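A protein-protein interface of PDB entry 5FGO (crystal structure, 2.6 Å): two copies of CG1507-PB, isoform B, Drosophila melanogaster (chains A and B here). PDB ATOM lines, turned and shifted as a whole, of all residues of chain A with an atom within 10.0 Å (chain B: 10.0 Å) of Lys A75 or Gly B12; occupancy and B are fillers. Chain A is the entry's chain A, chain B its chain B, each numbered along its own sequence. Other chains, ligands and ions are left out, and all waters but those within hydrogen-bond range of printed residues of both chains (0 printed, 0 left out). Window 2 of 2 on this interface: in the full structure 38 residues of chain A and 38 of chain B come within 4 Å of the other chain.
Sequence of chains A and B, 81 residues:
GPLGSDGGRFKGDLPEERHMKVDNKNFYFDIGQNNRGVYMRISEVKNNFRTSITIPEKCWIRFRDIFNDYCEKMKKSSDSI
SG of Cys A71 is in hydrogen-bond range of O of Trp B60, at 3.7 Å. The side-chain amino group of Lys A75 lies close to the backbone NH of Gly B12, at 3.0 Å.
O of Val B38 lies within hydrogen-bond range of N of Glu B57, 2.7 Å away.
CE1 of Tyr A70 touches CB of Pro B15 (3.6 Å). CD1 of Ile B31 touches CE1 of Tyr A70 (3.5 Å). Tyr A70 touches Trp B60 (O to CZ3, 3.8 Å). Lys A73 touches Pro B15. OE2 of Glu B57 touches CB of Met A74, at 3.3 Å. Met A74 touches Ile B61 (CE to CD1, 3.3 Å).
Lys A75 touches one residue of chain B. Of the printed residues of chain A, Gly B12 touches Lys A75 (3.0 Å). Printed residues of chain A within 4 Å of Pro B15: Tyr A70 (3.6 Å) and Lys A73 (3.8 Å). Gly B32 touches none of the printed residues of chain A. Of the printed residues of chain A, Glu B57 touches Met A74. Printed residues of chain A within 4 Å of Trp B60: Tyr A70 (3.8 Å) and Cys A71 (3.7 Å). The nearest residue of chain B that does not touch Lys A75 is Glu B57 (4.4 Å). The nearest residue of chain A that does not touch Gly B12 is Lys A76 (8.5 Å).
Printed residues of chain A that touch a printed residue of chain B: Tyr A70, Cys A71, Lys A73, Met A74 and Lys A75. Along chain A the printed residues that touch a printed residue of chain B span positions 70 to 75. Of the 12 printed residues of chain B, 6 touch a printed residue of chain A. Printed residues of chain B that touch a printed residue of chain A: Gly B12, Pro B15, Ile B31, Glu B57, Trp B60 and Ile B61. Hydrophobic or aromatic side chains of chain B within 4 Å of the printed part of chain A: Pro B15, Ile B31, Trp B60 and Ile B61. Among the printed residues, no Asp or Glu carboxylate lies within 4 Å of a Lys or Arg side-chain nitrogen of the other chain.
No position is printed for both chains.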
ATOM      1  N   ASP A  69       6.760  12.438  -8.065  1.00  0.00           N
ATOM      2  CA  ASP A  69       6.784  11.108  -7.464  1.00  0.00           C
ATOM      3  C   ASP A  69       6.842  11.211  -5.938  1.00  0.00           C
ATOM      4  O   ASP A  69       6.242  10.404  -5.225  1.00  0.00           O
ATOM      5  CB  ASP A  69       7.972  10.297  -7.976  1.00  0.00           C
ATOM      6  CG  ASP A  69       7.819   9.872  -9.429  1.00  0.00           C
ATOM      7  OD1 ASP A  69       6.693   9.894  -9.969  1.00  0.00           O
ATOM      8  OD2 ASP A  69       8.846   9.505 -10.033  1.00  0.00           O
ATOM      9  N   TYR A  70       7.605  12.181  -5.438  1.00  0.00           N
ATOM     10  CA  TYR A  70       7.686  12.440  -4.005  1.00  0.00           C
ATOM     11  C   TYR A  70       6.342  12.915  -3.508  1.00  0.00           C
ATOM     12  O   TYR A  70       5.930  12.570  -2.408  1.00  0.00           O
ATOM     13  CB  TYR A  70       8.758  13.478  -3.693  1.00  0.00           C
ATOM     14  CG  TYR A  70      10.146  12.901  -3.560  1.00  0.00           C
ATOM     15  CD1 TYR A  70      10.454  12.017  -2.536  1.00  0.00           C
ATOM     16  CD2 TYR A  70      11.128  13.191  -4.487  1.00  0.00           C
ATOM     17  CE1 TYR A  70      11.709  11.471  -2.413  1.00  0.00           C
ATOM     18  CE2 TYR A  70      12.377  12.640  -4.380  1.00  0.00           C
ATOM     19  CZ  TYR A  70      12.663  11.784  -3.340  1.00  0.00           C
ATOM     20  OH  TYR A  70      13.907  11.229  -3.233  1.00  0.00           O
ATOM     21  N   CYS A  71       5.658  13.727  -4.304  1.00  0.00           N
ATOM     22  CA  CYS A  71       4.330  14.146  -3.892  1.00  0.00           C
ATOM     23  C   CYS A  71       3.346  12.991  -3.926  1.00  0.00           C
ATOM     24  O   CYS A  71       2.327  13.026  -3.250  1.00  0.00           O
ATOM     25  CB  CYS A  71       3.785  15.249  -4.798  1.00  0.00           C
ATOM     26  SG  CYS A  71       4.554  16.848  -4.659  1.00  0.00           S
ATOM     27  N   GLU A  72       3.663  11.947  -4.677  1.00  0.00           N
ATOM     28  CA  GLU A  72       2.755  10.818  -4.742  1.00  0.00           C
ATOM     29  C   GLU A  72       2.897   9.887  -3.531  1.00  0.00           C
ATOM     30  O   GLU A  72       1.962   9.185  -3.192  1.00  0.00           O
ATOM     31  CB  GLU A  72       2.904  10.094  -6.087  1.00  0.00           C
ATOM     32  CG  GLU A  72       2.357  10.989  -7.211  1.00  0.00           C
ATOM     33  CD  GLU A  72       2.125  10.328  -8.566  1.00  0.00           C
ATOM     34  OE1 GLU A  72       2.420   9.122  -8.751  1.00  0.00           O
ATOM     35  OE2 GLU A  72       1.604  11.044  -9.459  1.00  0.00           O
ATOM     36  N   LYS A  73       4.042   9.918  -2.856  1.00  0.00           N
ATOM     37  CA  LYS A  73       4.278   9.064  -1.699  1.00  0.00           C
ATOM     38  C   LYS A  73       3.722   9.627  -0.398  1.00  0.00           C
ATOM     39  O   LYS A  73       3.759   8.928   0.617  1.00  0.00           O
ATOM     40  CB  LYS A  73       5.777   8.816  -1.460  1.00  0.00           C
ATOM     41  CG  LYS A  73       6.454   7.631  -2.135  1.00  0.00           C
ATOM     42  CD  LYS A  73       6.521   7.678  -3.647  1.00  0.00           C
ATOM     43  CE  LYS A  73       7.322   6.470  -4.157  1.00  0.00           C
ATOM     44  NZ  LYS A  73       7.531   6.421  -5.639  1.00  0.00           N
ATOM     45  N   MET A  74       3.233  10.869  -0.381  1.00  0.00           N
ATOM     46  CA  MET A  74       2.938  11.496   0.923  1.00  0.00           C
ATOM     47  C   MET A  74       1.642  10.988   1.562  1.00  0.00           C
ATOM     48  O   MET A  74       0.759  10.491   0.872  1.00  0.00           O
ATOM     49  CB  MET A  74       2.922  13.039   0.843  1.00  0.00           C
ATOM     50  CG  MET A  74       2.416  13.722  -0.424  1.00  0.00           C
ATOM     51  SD  MET A  74       2.734  15.706  -0.357  1.00  0.00           S
ATOM     52  CE  MET A  74       2.094  16.131  -2.081  1.00  0.00           C
ATOM     53  N   LYS A  75       1.569  11.100   2.891  1.00  0.00           N
ATOM     54  CA  LYS A  75       0.468  10.552   3.691  1.00  0.00           C
ATOM     55  C   LYS A  75      -0.303  11.604   4.514  1.00  0.00           C
ATOM     56  O   LYS A  75      -0.372  12.777   4.151  1.00  0.00           O
ATOM     57  CB  LYS A  75       1.004   9.482   4.658  1.00  0.00           C
ATOM     58  CG  LYS A  75       1.900  10.039   5.772  1.00  0.00           C
ATOM     59  CD  LYS A  75       2.280   8.969   6.795  1.00  0.00           C
ATOM     60  CE  LYS A  75       3.071   9.574   7.951  1.00  0.00           C
ATOM     61  NZ  LYS A  75       3.535   8.558   8.935  1.00  0.00           N
ATOM     62  N   LYS A  76      -0.906  11.134   5.608  1.00  0.00           N
ATOM     63  CA  LYS A  76      -1.560  11.955   6.625  1.00  0.00           C
ATOM     64  C   LYS A  76      -1.715  11.144   7.909  1.00  0.00           C
ATOM     65  O   LYS A  76      -2.704  10.434   8.091  1.00  0.00           O
ATOM     66  CB  LYS A  76      -2.921  12.486   6.165  1.00  0.00           C
ATOM     67  CG  LYS A  76      -3.561  13.448   7.176  1.00  0.00           C
ATOM     68  CD  LYS A  76      -4.737  14.235   6.603  1.00  0.00           C
ATOM     69  CE  LYS A  76      -5.454  15.054   7.685  1.00  0.00           C
ATOM     70  NZ  LYS A  76      -4.606  16.055   8.361  1.00  0.00           N
ATOM     71  N   GLY B  12       5.097   6.003   8.623  1.00  0.00           N
ATOM     72  CA  GLY B  12       5.871   4.950   7.985  1.00  0.00           C
ATOM     73  C   GLY B  12       7.286   5.420   7.721  1.00  0.00           C
ATOM     74  O   GLY B  12       7.721   6.425   8.287  1.00  0.00           O
ATOM     75  N   ASP B  13       8.017   4.704   6.873  1.00  0.00           N
ATOM     76  CA  ASP B  13       9.388   5.096   6.616  1.00  0.00           C
ATOM     77  C   ASP B  13       9.307   6.190   5.584  1.00  0.00           C
ATOM     78  O   ASP B  13       8.261   6.392   4.985  1.00  0.00           O
ATOM     79  CB  ASP B  13      10.240   3.931   6.123  1.00  0.00           C
ATOM     80  CG  ASP B  13      11.657   3.996   6.655  1.00  0.00           C
ATOM     81  OD1 ASP B  13      11.881   4.775   7.608  1.00  0.00           O
ATOM     82  OD2 ASP B  13      12.544   3.278   6.141  1.00  0.00           O
ATOM     83  N   LEU B  14      10.417   6.863   5.328  1.00  0.00           N
ATOM     84  CA  LEU B  14      10.411   7.960   4.370  1.00  0.00           C
ATOM     85  C   LEU B  14      10.683   7.452   2.971  1.00  0.00           C
ATOM     86  O   LEU B  14      11.251   6.379   2.809  1.00  0.00           O
ATOM     87  CB  LEU B  14      11.447   9.002   4.779  1.00  0.00           C
ATOM     88  CG  LEU B  14      11.216   9.564   6.189  1.00  0.00           C
ATOM     89  CD1 LEU B  14      12.370  10.481   6.636  1.00  0.00           C
ATOM     90  CD2 LEU B  14       9.870  10.264   6.261  1.00  0.00           C
ATOM     91  N   PRO B  15      10.225   8.186   1.951  1.00  0.00           N
ATOM     92  CA  PRO B  15      10.564   7.913   0.547  1.00  0.00           C
ATOM     93  C   PRO B  15      12.085   7.764   0.355  1.00  0.00           C
ATOM     94  O   PRO B  15      12.843   8.290   1.182  1.00  0.00           O
ATOM     95  CB  PRO B  15      10.015   9.144  -0.185  1.00  0.00           C
ATOM     96  CG  PRO B  15       8.870   9.562   0.636  1.00  0.00           C
ATOM     97  CD  PRO B  15       9.224   9.258   2.069  1.00  0.00           C
ATOM     98  N   ILE B  31      14.968  12.712   1.745  1.00  0.00           N
ATOM     99  CA  ILE B  31      13.956  13.074   2.704  1.00  0.00           C
ATOM    100  C   ILE B  31      14.456  12.965   4.152  1.00  0.00           C
ATOM    101  O   ILE B  31      15.237  12.090   4.484  1.00  0.00           O
ATOM    102  CB  ILE B  31      12.707  12.187   2.515  1.00  0.00           C
ATOM    103  CG1 ILE B  31      12.312  12.154   1.040  1.00  0.00           C
ATOM    104  CG2 ILE B  31      11.561  12.610   3.421  1.00  0.00           C
ATOM    105  CD1 ILE B  31      11.964  13.473   0.483  1.00  0.00           C
ATOM    106  N   GLY B  32      14.104  13.936   4.987  1.00  0.00           N
ATOM    107  CA  GLY B  32      14.438  13.868   6.399  1.00  0.00           C
ATOM    108  C   GLY B  32      13.312  14.422   7.255  1.00  0.00           C
ATOM    109  O   GLY B  32      12.328  14.965   6.727  1.00  0.00           O
ATOM    110  N   GLN B  33      13.429  14.275   8.572  1.00  0.00           N
ATOM    111  CA  GLN B  33      12.404  14.829   9.444  1.00  0.00           C
ATOM    112  C   GLN B  33      12.970  15.212  10.817  1.00  0.00           C
ATOM    113  O   GLN B  33      13.791  14.498  11.385  1.00  0.00           O
ATOM    114  CB  GLN B  33      11.218  13.865   9.622  1.00  0.00           C
ATOM    115  CG  GLN B  33      11.455  12.690  10.536  1.00  0.00           C
ATOM    116  CD  GLN B  33      10.183  11.921  10.835  1.00  0.00           C
ATOM    117  OE1 GLN B  33       9.162  12.109  10.174  1.00  0.00           O
ATOM    118  NE2 GLN B  33      10.225  11.080  11.863  1.00  0.00           N
ATOM    119  N   VAL B  38       8.726  16.966   8.264  1.00  0.00           N
ATOM    120  CA  VAL B  38       9.326  16.308   7.112  1.00  0.00           C
ATOM    121  C   VAL B  38       9.736  17.310   6.021  1.00  0.00           C
ATOM    122  O   VAL B  38       8.982  18.216   5.670  1.00  0.00           O
ATOM    123  CB  VAL B  38       8.319  15.286   6.527  1.00  0.00           C
ATOM    124  CG1 VAL B  38       8.810  14.697   5.223  1.00  0.00           C
ATOM    125  CG2 VAL B  38       8.040  14.201   7.535  1.00  0.00           C
ATOM    126  N   GLU B  57       7.525  19.720   3.939  1.00  0.00           N
ATOM    127  CA  GLU B  57       6.451  18.974   3.285  1.00  0.00           C
ATOM    128  C   GLU B  57       5.206  19.813   3.018  1.00  0.00           C
ATOM    129  O   GLU B  57       4.640  19.727   1.941  1.00  0.00           O
ATOM    130  CB  GLU B  57       6.044  17.741   4.098  1.00  0.00           C
ATOM    131  CG  GLU B  57       5.184  16.768   3.269  1.00  0.00           C
ATOM    132  CD  GLU B  57       4.585  15.598   4.055  1.00  0.00           C
ATOM    133  OE1 GLU B  57       4.822  15.476   5.280  1.00  0.00           O
ATOM    134  OE2 GLU B  57       3.864  14.791   3.426  1.00  0.00           O
ATOM    135  N   LYS B  58       4.824  20.688   3.942  1.00  0.00           N
ATOM    136  CA  LYS B  58       3.560  21.423   3.814  1.00  0.00           C
ATOM    137  C   LYS B  58       3.471  22.282   2.555  1.00  0.00           C
ATOM    138  O   LYS B  58       2.443  22.911   2.302  1.00  0.00           O
ATOM    139  CB  LYS B  58       3.322  22.309   5.030  1.00  0.00           C
ATOM    140  CG  LYS B  58       4.286  23.461   5.139  1.00  0.00           C
ATOM    141  CD  LYS B  58       3.995  24.356   6.314  1.00  0.00           C
ATOM    142  CE  LYS B  58       4.492  23.728   7.589  1.00  0.00           C
ATOM    143  NZ  LYS B  58       4.478  24.678   8.756  1.00  0.00           N
ATOM    144  N   TRP B  60       5.061  21.019  -0.605  1.00  0.00           N
ATOM    145  CA  TRP B  60       5.447  20.202  -1.773  1.00  0.00           C
ATOM    146  C   TRP B  60       4.459  20.391  -2.941  1.00  0.00           C
ATOM    147  O   TRP B  60       4.880  20.462  -4.106  1.00  0.00           O
ATOM    148  CB  TRP B  60       5.554  18.702  -1.415  1.00  0.00           C
ATOM    149  CG  TRP B  60       6.729  18.407  -0.517  1.00  0.00           C
ATOM    150  CD1 TRP B  60       7.593  19.322   0.016  1.00  0.00           C
ATOM    151  CD2 TRP B  60       7.212  17.117  -0.106  1.00  0.00           C
ATOM    152  NE1 TRP B  60       8.545  18.686   0.771  1.00  0.00           N
ATOM    153  CE2 TRP B  60       8.343  17.336   0.703  1.00  0.00           C
ATOM    154  CE3 TRP B  60       6.793  15.805  -0.337  1.00  0.00           C
ATOM    155  CZ2 TRP B  60       9.056  16.294   1.289  1.00  0.00           C
ATOM    156  CZ3 TRP B  60       7.509  14.759   0.245  1.00  0.00           C
ATOM    157  CH2 TRP B  60       8.628  15.014   1.047  1.00  0.00           C
ATOM    158  N   ILE B  61       3.159  20.463  -2.637  1.00  0.00           N
ATOM    159  CA  ILE B  61       2.160  20.646  -3.687  1.00  0.00           C
ATOM    160  C   ILE B  61       2.303  21.996  -4.379  1.00  0.00           C
ATOM    161  O   ILE B  61       2.290  22.078  -5.613  1.00  0.00           O
ATOM    162  CB  ILE B  61       0.726  20.491  -3.155  1.00  0.00           C
ATOM    163  CG1 ILE B  61       0.438  19.026  -2.847  1.00  0.00           C
ATOM    164  CG2 ILE B  61      -0.282  20.920  -4.222  1.00  0.00           C
ATOM    165  CD1 ILE B  61       0.401  18.183  -4.104  1.00  0.00           C
